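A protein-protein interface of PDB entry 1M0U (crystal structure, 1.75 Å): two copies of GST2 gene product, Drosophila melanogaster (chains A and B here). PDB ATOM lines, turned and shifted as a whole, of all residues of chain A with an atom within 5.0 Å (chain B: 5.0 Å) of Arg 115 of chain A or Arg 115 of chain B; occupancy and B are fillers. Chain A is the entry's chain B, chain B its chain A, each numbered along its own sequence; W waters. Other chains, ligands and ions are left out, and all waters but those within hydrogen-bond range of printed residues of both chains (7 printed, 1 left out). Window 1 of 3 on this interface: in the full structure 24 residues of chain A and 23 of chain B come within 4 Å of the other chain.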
ATOM      1  N   ILE A 111     -14.142  11.290  -2.186  1.00  0.00           N
ATOM      2  CA  ILE A 111     -14.928  10.541  -1.188  1.00  0.00           C
ATOM      3  C   ILE A 111     -14.030   9.500  -0.529  1.00  0.00           C
ATOM      4  O   ILE A 111     -14.022   9.343   0.709  1.00  0.00           O
ATOM      5  CB  ILE A 111     -16.190   9.879  -1.808  1.00  0.00           C
ATOM      6  CG1 ILE A 111     -17.105  10.919  -2.460  1.00  0.00           C
ATOM      7  CG2 ILE A 111     -16.959   9.065  -0.738  1.00  0.00           C
ATOM      8  CD1 ILE A 111     -17.679  11.901  -1.517  1.00  0.00           C
ATOM      9  N   SER A 112     -13.261   8.785  -1.351  1.00  0.00           N
ATOM     10  CA  SER A 112     -12.389   7.770  -0.800  1.00  0.00           C
ATOM     11  C   SER A 112     -11.262   8.393   0.050  1.00  0.00           C
ATOM     12  O   SER A 112     -10.864   7.810   1.055  1.00  0.00           O
ATOM     13  CB  SER A 112     -11.864   6.843  -1.886  1.00  0.00           C
ATOM     14  OG  SER A 112     -12.913   5.933  -2.225  1.00  0.00           O
ATOM     15  N   MET A 113     -10.781   9.575  -0.345  1.00  0.00           N
ATOM     16  CA  MET A 113      -9.776  10.287   0.465  1.00  0.00           C
ATOM     17  C   MET A 113     -10.392  10.761   1.786  1.00  0.00           C
ATOM     18  O   MET A 113      -9.735  10.707   2.842  1.00  0.00           O
ATOM     19  CB  MET A 113      -9.153  11.453  -0.313  1.00  0.00           C
ATOM     20  CG  MET A 113      -8.353  10.939  -1.494  1.00  0.00           C
ATOM     21  SD  MET A 113      -7.428  12.276  -2.278  1.00  0.00           S
ATOM     22  CE  MET A 113      -8.690  13.251  -2.927  1.00  0.00           C
ATOM     23  N   ALA A 114     -11.650  11.195   1.739  1.00  0.00           N
ATOM     24  CA  ALA A 114     -12.328  11.580   2.987  1.00  0.00           C
ATOM     25  C   ALA A 114     -12.422  10.372   3.918  1.00  0.00           C
ATOM     26  O   ALA A 114     -12.188  10.502   5.119  1.00  0.00           O
ATOM     27  CB  ALA A 114     -13.723  12.156   2.712  1.00  0.00           C
ATOM     28  N   ARG A 115     -12.802   9.216   3.374  1.00  0.00           N
ATOM     29  CA  ARG A 115     -12.905   7.982   4.171  1.00  0.00           C
ATOM     30  C   ARG A 115     -11.561   7.640   4.826  1.00  0.00           C
ATOM     31  O   ARG A 115     -11.516   7.209   5.979  1.00  0.00           O
ATOM     32  CB  ARG A 115     -13.404   6.820   3.315  1.00  0.00           C
ATOM     33  CG  ARG A 115     -13.618   5.456   4.037  1.00  0.00           C
ATOM     34  CD  ARG A 115     -14.027   4.276   3.079  1.00  0.00           C
ATOM     35  NE  ARG A 115     -15.184   4.691   2.289  1.00  0.00           N
ATOM     36  CZ  ARG A 115     -15.155   4.973   0.986  1.00  0.00           C
ATOM     37  NH1 ARG A 115     -14.037   4.801   0.271  1.00  0.00           N
ATOM     38  NH2 ARG A 115     -16.266   5.411   0.387  1.00  0.00           N
ATOM     39  N   PHE A 116     -10.472   7.806   4.070  1.00  0.00           N
ATOM     40  CA  PHE A 116      -9.144   7.586   4.619  1.00  0.00           C
ATOM     41  C   PHE A 116      -8.807   8.574   5.750  1.00  0.00           C
ATOM     42  O   PHE A 116      -8.329   8.163   6.847  1.00  0.00           O
ATOM     43  CB  PHE A 116      -8.105   7.671   3.495  1.00  0.00           C
ATOM     44  CG  PHE A 116      -6.695   7.780   4.015  1.00  0.00           C
ATOM     45  CD1 PHE A 116      -6.057   6.650   4.543  1.00  0.00           C
ATOM     46  CD2 PHE A 116      -6.037   8.997   3.982  1.00  0.00           C
ATOM     47  CE1 PHE A 116      -4.749   6.743   5.037  1.00  0.00           C
ATOM     48  CE2 PHE A 116      -4.719   9.107   4.468  1.00  0.00           C
ATOM     49  CZ  PHE A 116      -4.088   7.987   4.991  1.00  0.00           C
ATOM     50  N   LEU A 117      -9.044   9.856   5.508  1.00  0.00           N
ATOM     51  CA  LEU A 117      -8.805  10.866   6.554  1.00  0.00           C
ATOM     52  C   LEU A 117      -9.666  10.601   7.787  1.00  0.00           C
ATOM     53  O   LEU A 117      -9.203  10.782   8.932  1.00  0.00           O
ATOM     54  CB  LEU A 117      -9.051  12.273   6.041  1.00  0.00           C
ATOM     55  CG  LEU A 117      -8.033  12.786   5.026  1.00  0.00           C
ATOM     56  CD1 LEU A 117      -8.368  14.213   4.749  1.00  0.00           C
ATOM     57  CD2 LEU A 117      -6.582  12.684   5.624  1.00  0.00           C
ATOM     58  N   ALA A 118     -10.890  10.136   7.556  1.00  0.00           N
ATOM     59  CA  ALA A 118     -11.781   9.828   8.692  1.00  0.00           C
ATOM     60  C   ALA A 118     -11.203   8.699   9.542  1.00  0.00           C
ATOM     61  O   ALA A 118     -11.223   8.753  10.779  1.00  0.00           O
ATOM     62  CB  ALA A 118     -13.159   9.453   8.166  1.00  0.00           C
ATOM     63  N   LYS A 119     -10.657   7.679   8.884  1.00  0.00           N
ATOM     64  CA  LYS A 119      -9.993   6.590   9.616  1.00  0.00           C
ATOM     65  C   LYS A 119      -8.856   7.093  10.477  1.00  0.00           C
ATOM     66  O   LYS A 119      -8.718   6.668  11.629  1.00  0.00           O
ATOM     67  CB  LYS A 119      -9.454   5.533   8.679  1.00  0.00           C
ATOM     68  CG  LYS A 119     -10.509   4.628   8.142  1.00  0.00           C
ATOM     69  CD  LYS A 119      -9.939   3.801   6.994  1.00  0.00           C
ATOM     70  CE  LYS A 119     -11.068   3.337   6.107  1.00  0.00           C
ATOM     71  NZ  LYS A 119     -10.628   2.414   5.026  1.00  0.00           N
ATOM     72  N   CYS A 124     -14.604   6.966  11.904  1.00  0.00           N
ATOM     73  CA  CYS A 124     -15.307   5.846  11.305  1.00  0.00           C
ATOM     74  C   CYS A 124     -15.998   4.968  12.334  1.00  0.00           C
ATOM     75  O   CYS A 124     -16.368   5.452  13.410  1.00  0.00           O
ATOM     76  CB  CYS A 124     -14.362   5.046  10.427  1.00  0.00           C
ATOM     77  SG  CYS A 124     -13.892   6.021   8.993  1.00  0.00           S
ATOM     78  N   ASP A 135     -20.553   4.571   5.009  1.00  0.00           N
ATOM     79  CA  ASP A 135     -20.264   4.598   3.564  1.00  0.00           C
ATOM     80  C   ASP A 135     -21.554   4.805   2.771  1.00  0.00           C
ATOM     81  O   ASP A 135     -21.591   5.611   1.833  1.00  0.00           O
ATOM     82  CB  ASP A 135     -19.612   3.298   3.108  1.00  0.00           C
ATOM     83  CG  ASP A 135     -18.125   3.230   3.423  1.00  0.00           C
ATOM     84  OD1 ASP A 135     -17.518   4.257   3.798  1.00  0.00           O
ATOM     85  OD2 ASP A 135     -17.476   2.172   3.290  1.00  0.00           O
ATOM     86  N   ASP A 139     -22.424   7.851   0.264  1.00  0.00           N
ATOM     87  CA  ASP A 139     -22.714   7.546  -1.152  1.00  0.00           C
ATOM     88  C   ASP A 139     -24.031   8.212  -1.563  1.00  0.00           C
ATOM     89  O   ASP A 139     -24.153   8.767  -2.658  1.00  0.00           O
ATOM     90  CB  ASP A 139     -22.870   6.051  -1.384  1.00  0.00           C
ATOM     91  CG  ASP A 139     -21.572   5.290  -1.325  1.00  0.00           C
ATOM     92  OD1 ASP A 139     -20.469   5.887  -1.421  1.00  0.00           O
ATOM     93  OD2 ASP A 139     -21.587   4.041  -1.213  1.00  0.00           O
ATOM     94  N   TRP A 197     -17.745  10.555  10.126  1.00  0.00           N
ATOM     95  CA  TRP A 197     -17.342  11.416   9.015  1.00  0.00           C
ATOM     96  C   TRP A 197     -18.482  11.729   8.041  1.00  0.00           C
ATOM     97  O   TRP A 197     -18.368  12.672   7.243  1.00  0.00           O
ATOM     98  CB  TRP A 197     -16.137  10.866   8.271  1.00  0.00           C
ATOM     99  CG  TRP A 197     -16.341   9.621   7.474  1.00  0.00           C
ATOM    100  CD1 TRP A 197     -16.394   8.339   7.952  1.00  0.00           C
ATOM    101  CD2 TRP A 197     -16.482   9.523   6.048  1.00  0.00           C
ATOM    102  NE1 TRP A 197     -16.543   7.448   6.912  1.00  0.00           N
ATOM    103  CE2 TRP A 197     -16.606   8.153   5.731  1.00  0.00           C
ATOM    104  CE3 TRP A 197     -16.500  10.459   5.000  1.00  0.00           C
ATOM    105  CZ2 TRP A 197     -16.760   7.680   4.408  1.00  0.00           C
ATOM    106  CZ3 TRP A 197     -16.643   9.979   3.671  1.00  0.00           C
ATOM    107  CH2 TRP A 197     -16.781   8.620   3.397  1.00  0.00           C
ATOM    108  N   ILE B 111     -21.245  -0.401  -4.619  1.00  0.00           N
ATOM    109  CA  ILE B 111     -19.798  -0.277  -4.400  1.00  0.00           C
ATOM    110  C   ILE B 111     -19.473  -0.404  -2.903  1.00  0.00           C
ATOM    111  O   ILE B 111     -18.546  -1.119  -2.512  1.00  0.00           O
ATOM    112  CB  ILE B 111     -19.220   1.051  -4.936  1.00  0.00           C
ATOM    113  CG1 ILE B 111     -19.460   1.189  -6.454  1.00  0.00           C
ATOM    114  CG2 ILE B 111     -17.719   1.155  -4.579  1.00  0.00           C
ATOM    115  CD1 ILE B 111     -18.960   0.021  -7.224  1.00  0.00           C
ATOM    116  N   SER B 112     -20.251   0.278  -2.075  1.00  0.00           N
ATOM    117  CA  SER B 112     -19.996   0.195  -0.634  1.00  0.00           C
ATOM    118  C   SER B 112     -20.273  -1.204  -0.081  1.00  0.00           C
ATOM    119  O   SER B 112     -19.548  -1.680   0.804  1.00  0.00           O
ATOM    120  CB  SER B 112     -20.765   1.282   0.091  1.00  0.00           C
ATOM    121  OG  SER B 112     -20.077   2.516  -0.102  1.00  0.00           O
ATOM    122  N   MET B 113     -21.291  -1.877  -0.625  1.00  0.00           N
ATOM    123  CA  MET B 113     -21.523  -3.272  -0.255  1.00  0.00           C
ATOM    124  C   MET B 113     -20.413  -4.213  -0.714  1.00  0.00           C
ATOM    125  O   MET B 113     -20.098  -5.166  -0.015  1.00  0.00           O
ATOM    126  CB  MET B 113     -22.896  -3.752  -0.731  1.00  0.00           C
ATOM    127  CG  MET B 113     -24.032  -2.927  -0.133  1.00  0.00           C
ATOM    128  SD  MET B 113     -25.623  -3.723  -0.473  1.00  0.00           S
ATOM    129  CE  MET B 113     -25.762  -3.444  -2.279  1.00  0.00           C
ATOM    130  N   ALA B 114     -19.818  -3.953  -1.883  1.00  0.00           N
ATOM    131  CA  ALA B 114     -18.692  -4.747  -2.348  1.00  0.00           C
ATOM    132  C   ALA B 114     -17.511  -4.586  -1.394  1.00  0.00           C
ATOM    133  O   ALA B 114     -16.810  -5.559  -1.088  1.00  0.00           O
ATOM    134  CB  ALA B 114     -18.292  -4.317  -3.799  1.00  0.00           C
ATOM    135  N   ARG B 115     -17.284  -3.358  -0.921  1.00  0.00           N
ATOM    136  CA  ARG B 115     -16.154  -3.077  -0.039  1.00  0.00           C
ATOM    137  C   ARG B 115     -16.379  -3.849   1.260  1.00  0.00           C
ATOM    138  O   ARG B 115     -15.446  -4.430   1.806  1.00  0.00           O
ATOM    139  CB  ARG B 115     -16.066  -1.579   0.241  1.00  0.00           C
ATOM    140  CG  ARG B 115     -14.896  -1.141   1.147  1.00  0.00           C
ATOM    141  CD  ARG B 115     -14.889   0.357   1.458  1.00  0.00           C
ATOM    142  NE  ARG B 115     -14.900   1.124   0.214  1.00  0.00           N
ATOM    143  CZ  ARG B 115     -15.919   1.822  -0.248  1.00  0.00           C
ATOM    144  NH1 ARG B 115     -17.056   1.943   0.442  1.00  0.00           N
ATOM    145  NH2 ARG B 115     -15.806   2.411  -1.448  1.00  0.00           N
ATOM    146  N   PHE B 116     -17.630  -3.864   1.717  1.00  0.00           N
ATOM    147  CA  PHE B 116     -17.990  -4.604   2.940  1.00  0.00           C
ATOM    148  C   PHE B 116     -17.787  -6.118   2.759  1.00  0.00           C
ATOM    149  O   PHE B 116     -17.176  -6.782   3.602  1.00  0.00           O
ATOM    150  CB  PHE B 116     -19.436  -4.280   3.363  1.00  0.00           C
ATOM    151  CG  PHE B 116     -20.002  -5.274   4.349  1.00  0.00           C
ATOM    152  CD1 PHE B 116     -19.579  -5.260   5.684  1.00  0.00           C
ATOM    153  CD2 PHE B 116     -20.924  -6.226   3.932  1.00  0.00           C
ATOM    154  CE1 PHE B 116     -20.083  -6.198   6.594  1.00  0.00           C
ATOM    155  CE2 PHE B 116     -21.440  -7.178   4.829  1.00  0.00           C
ATOM    156  CZ  PHE B 116     -21.021  -7.154   6.166  1.00  0.00           C
ATOM    157  N   LEU B 117     -18.318  -6.690   1.682  1.00  0.00           N
ATOM    158  CA  LEU B 117     -18.046  -8.104   1.392  1.00  0.00           C
ATOM    159  C   LEU B 117     -16.552  -8.413   1.252  1.00  0.00           C
ATOM    160  O   LEU B 117     -16.081  -9.440   1.735  1.00  0.00           O
ATOM    161  CB  LEU B 117     -18.820  -8.567   0.146  1.00  0.00           C
ATOM    162  CG  LEU B 117     -20.339  -8.522   0.276  1.00  0.00           C
ATOM    163  CD1 LEU B 117     -20.982  -9.018  -1.026  1.00  0.00           C
ATOM    164  CD2 LEU B 117     -20.838  -9.371   1.485  1.00  0.00           C
ATOM    165  N   ALA B 118     -15.797  -7.511   0.617  1.00  0.00           N
ATOM    166  CA  ALA B 118     -14.348  -7.659   0.472  1.00  0.00           C
ATOM    167  C   ALA B 118     -13.653  -7.816   1.845  1.00  0.00           C
ATOM    168  O   ALA B 118     -12.777  -8.664   2.027  1.00  0.00           O
ATOM    169  CB  ALA B 118     -13.776  -6.435  -0.261  1.00  0.00           C
ATOM    170  N   LYS B 119     -14.062  -6.994   2.805  1.00  0.00           N
ATOM    171  CA  LYS B 119     -13.502  -7.064   4.151  1.00  0.00           C
ATOM    172  C   LYS B 119     -13.874  -8.401   4.761  1.00  0.00           C
ATOM    173  O   LYS B 119     -13.049  -9.038   5.427  1.00  0.00           O
ATOM    174  CB  LYS B 119     -14.053  -5.941   5.027  1.00  0.00           C
ATOM    175  CG  LYS B 119     -13.449  -4.608   4.744  1.00  0.00           C
ATOM    176  CD  LYS B 119     -14.212  -3.506   5.445  1.00  0.00           C
ATOM    177  CE  LYS B 119     -14.000  -2.177   4.757  1.00  0.00           C
ATOM    178  NZ  LYS B 119     -14.789  -1.085   5.365  1.00  0.00           N
ATOM    179  N   CYS B 124      -8.974  -7.092   1.192  1.00  0.00           N
ATOM    180  CA  CYS B 124      -8.573  -5.707   1.400  1.00  0.00           C
ATOM    181  C   CYS B 124      -7.076  -5.566   1.662  1.00  0.00           C
ATOM    182  O   CYS B 124      -6.307  -6.488   1.389  1.00  0.00           O
ATOM    183  CB  CYS B 124      -9.428  -5.088   2.503  1.00  0.00           C
ATOM    184  SG  CYS B 124     -11.146  -4.973   1.977  1.00  0.00           S
ATOM    185  N   ASP B 135      -9.726   1.429  -2.889  1.00  0.00           N
ATOM    186  CA  ASP B 135     -10.936   2.235  -3.039  1.00  0.00           C
ATOM    187  C   ASP B 135     -10.852   3.145  -4.269  1.00  0.00           C
ATOM    188  O   ASP B 135     -11.818   3.289  -5.029  1.00  0.00           O
ATOM    189  CB  ASP B 135     -11.154   3.118  -1.815  1.00  0.00           C
ATOM    190  CG  ASP B 135     -11.784   2.378  -0.650  1.00  0.00           C
ATOM    191  OD1 ASP B 135     -12.291   1.246  -0.812  1.00  0.00           O
ATOM    192  OD2 ASP B 135     -11.785   2.884   0.493  1.00  0.00           O
ATOM    193  N   ASP B 139     -13.378   3.332  -7.425  1.00  0.00           N
ATOM    194  CA  ASP B 139     -14.133   4.552  -7.686  1.00  0.00           C
ATOM    195  C   ASP B 139     -13.925   4.952  -9.151  1.00  0.00           C
ATOM    196  O   ASP B 139     -14.843   5.425  -9.822  1.00  0.00           O
ATOM    197  CB  ASP B 139     -13.633   5.709  -6.850  1.00  0.00           C
ATOM    198  CG  ASP B 139     -14.071   5.643  -5.413  1.00  0.00           C
ATOM    199  OD1 ASP B 139     -15.016   4.893  -5.055  1.00  0.00           O
ATOM    200  OD2 ASP B 139     -13.528   6.385  -4.585  1.00  0.00           O
ATOM    201  N   TRP B 197      -9.907  -6.797  -3.898  1.00  0.00           N
ATOM    202  CA  TRP B 197     -11.271  -6.776  -4.391  1.00  0.00           C
ATOM    203  C   TRP B 197     -11.447  -5.870  -5.615  1.00  0.00           C
ATOM    204  O   TRP B 197     -12.470  -5.958  -6.280  1.00  0.00           O
ATOM    205  CB  TRP B 197     -12.277  -6.444  -3.274  1.00  0.00           C
ATOM    206  CG  TRP B 197     -12.269  -5.050  -2.757  1.00  0.00           C
ATOM    207  CD1 TRP B 197     -11.430  -4.524  -1.817  1.00  0.00           C
ATOM    208  CD2 TRP B 197     -13.191  -4.003  -3.098  1.00  0.00           C
ATOM    209  NE1 TRP B 197     -11.757  -3.212  -1.571  1.00  0.00           N
ATOM    210  CE2 TRP B 197     -12.826  -2.862  -2.353  1.00  0.00           C
ATOM    211  CE3 TRP B 197     -14.287  -3.907  -3.978  1.00  0.00           C
ATOM    212  CZ2 TRP B 197     -13.513  -1.642  -2.448  1.00  0.00           C
ATOM    213  CZ3 TRP B 197     -14.981  -2.698  -4.054  1.00  0.00           C
ATOM    214  CH2 TRP B 197     -14.590  -1.581  -3.300  1.00  0.00           C
HETATM  215  O   HOH W   1     -11.877   1.450   2.780  1.00  0.00           O
HETATM  216  O   HOH W   2     -18.432  -0.475   3.166  1.00  0.00           O
HETATM  217  O   HOH W   3     -13.015   0.977   5.204  1.00  0.00           O
HETATM  218  O   HOH W   4     -16.229   5.690  -2.606  1.00  0.00           O
HETATM  219  O   HOH W   5     -18.243   4.107  -2.373  1.00  0.00           O
HETATM  220  O   HOH W   6     -15.300   1.600   4.763  1.00  0.00           O
HETATM  221  O   HOH W   7     -10.283   5.016   1.567  1.00  0.00           O
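Water W6 lies within hydrogen-bond range of the side-chain carboxylate (OD2) of Asp 135 of chain A (2.7 Å) and the side-chain amino group (NZ) of Lys 119 of chain B (2.8 Å).
Water W1 lies within hydrogen-bond range of the side-chain carboxylate (OD2) of Asp 135 of chain B (2.7 Å) and the side-chain amino group (NZ) of Lys 119 of chain A (2.7 Å).
Water W2 bridges the side-chain carboxylate (OD2) of Asp 135 of chain A and the backbone carbonyl oxygen (O) of Ser 112 of chain B.
Water W7 bridges the side-chain carboxylate of Asp 135 of chain B (2.8 Å) and the backbone carbonyl oxygen of Ser 112 of chain A (2.9 Å).
Water W4 lies within hydrogen-bond range of the side-chain carboxylate of Asp 139 of chain B (2.8 Å), the guanidinium group of Arg 115 of chain A (3.0 Å) and the side-chain hydroxyl of Ser 112 of chain A (3.3 Å).
Water W5 lies within hydrogen-bond range of the side-chain carboxylate (OD1) of Asp 139 of chain A (3.0 Å), the guanidinium group (NH2) of Arg 115 of chain B (3.1 Å) and the side-chain hydroxyl (OG) of Ser 112 of chain B (3.3 Å).
Of chain B, only Arg 115 and Asp 135 come within 4 Å of Arg 115 of chain A.
Of the printed residues of chain A, Ser 112 of chain B touches Asp 135 and Asp 139.
Of chain A, only Arg 115 (3.4 Å) and Asp 135 (2.9 Å) come within 4 Å of Arg 115 of chain B.
Printed residues of chain A within 4 Å of Asp 135 of chain B: Ser 112 and Arg 115.
The nearest residue of chain B that does not touch Arg 115 of chain A is Ser 112 of chain B (4.8 Å).
The side-chain hydroxyl of Ser 112 of chain B sits at hydrogen-bond distance from the guanidinium group of Arg 115 of chain B (3.1 Å).
NE of Arg 115 of chain B is in salt-bridge range of OD1 of Asp 135 of chain B.
NE of Arg 115 of chain A is in salt-bridge range of OD1 of Asp 135 of chain A, 2.8 Å away.
NH1 of Arg 115 of chain A is in hydrogen-bond range of OG of Ser 112 of chain A (3.0 Å).
Among the printed residues, merely in contact across the chains: Ser 112 of chain A with Asp 135 of chain B (3.3 Å) and Asp 135 of chain A with Ser 112 of chain B (3.3 Å).
The side-chain hydroxyl of Ser 112 of chain A is in hydrogen-bond range of the side-chain carboxylate of Asp 139 of chain B (2.5 Å).
The side-chain hydroxyl (OG) of Ser 112 of chain B lies within hydrogen-bond range of the side-chain carboxylate (OD2) of Asp 139 of chain A (2.4 Å).
The guanidinium group of Arg 115 of chain B is in salt-bridge range of the side-chain carboxylate of Asp 135 of chain A (2.9 Å).
The guanidinium group of Arg 115 of chain A lies close to the guanidinium group of Arg 115 of chain B (3.4 Å).
The side-chain carboxylate (OD2) of Asp 135 of chain B lies within salt-bridge range of the guanidinium group (NH1) of Arg 115 of chain A (3.0 Å).
Ser 112 of chain A touches Asp 135 of chain B, and with the chains exchanged Asp 135 of chain A touches Ser 112 of chain B.
Ser 112 of chain A touches Asp 139 of chain B, and with the chains exchanged Asp 139 of chain A touches Ser 112 of chain B.
Arg 115 of chain B touches its own counterpart, Arg 115 of chain A.
Arg 115 of chain A touches Asp 135 of chain B, and with the chains exchanged Asp 135 of chain A touches Arg 115 of chain B.
Positions printed for both chains: 111, 112, 113, 114, 115, 116, 117, 118, 119, 124, 135, 139 and 197.
Of the 7 pairs that touch across the chains among the printed residues, 7 have their exchanged pair printed and touching as well.
Printed residues of chain A that touch a printed residue of chain B: Ser 112, Arg 115, Asp 135 and Asp 139.
Printed residues of chain B that touch a printed residue of chain A: Ser 112, Arg 115, Asp 135 and Asp 139.
Among the printed residues, 7 pairs touch across the chains.
Among the printed residues, Asp or Glu carboxylates within 4 Å of a Lys or Arg side-chain nitrogen of the other chain: Arg 115 of chain A with Asp 135 of chain B (3.0 Å) and Asp 135 of chain A with Arg 115 of chain B (2.9 Å).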
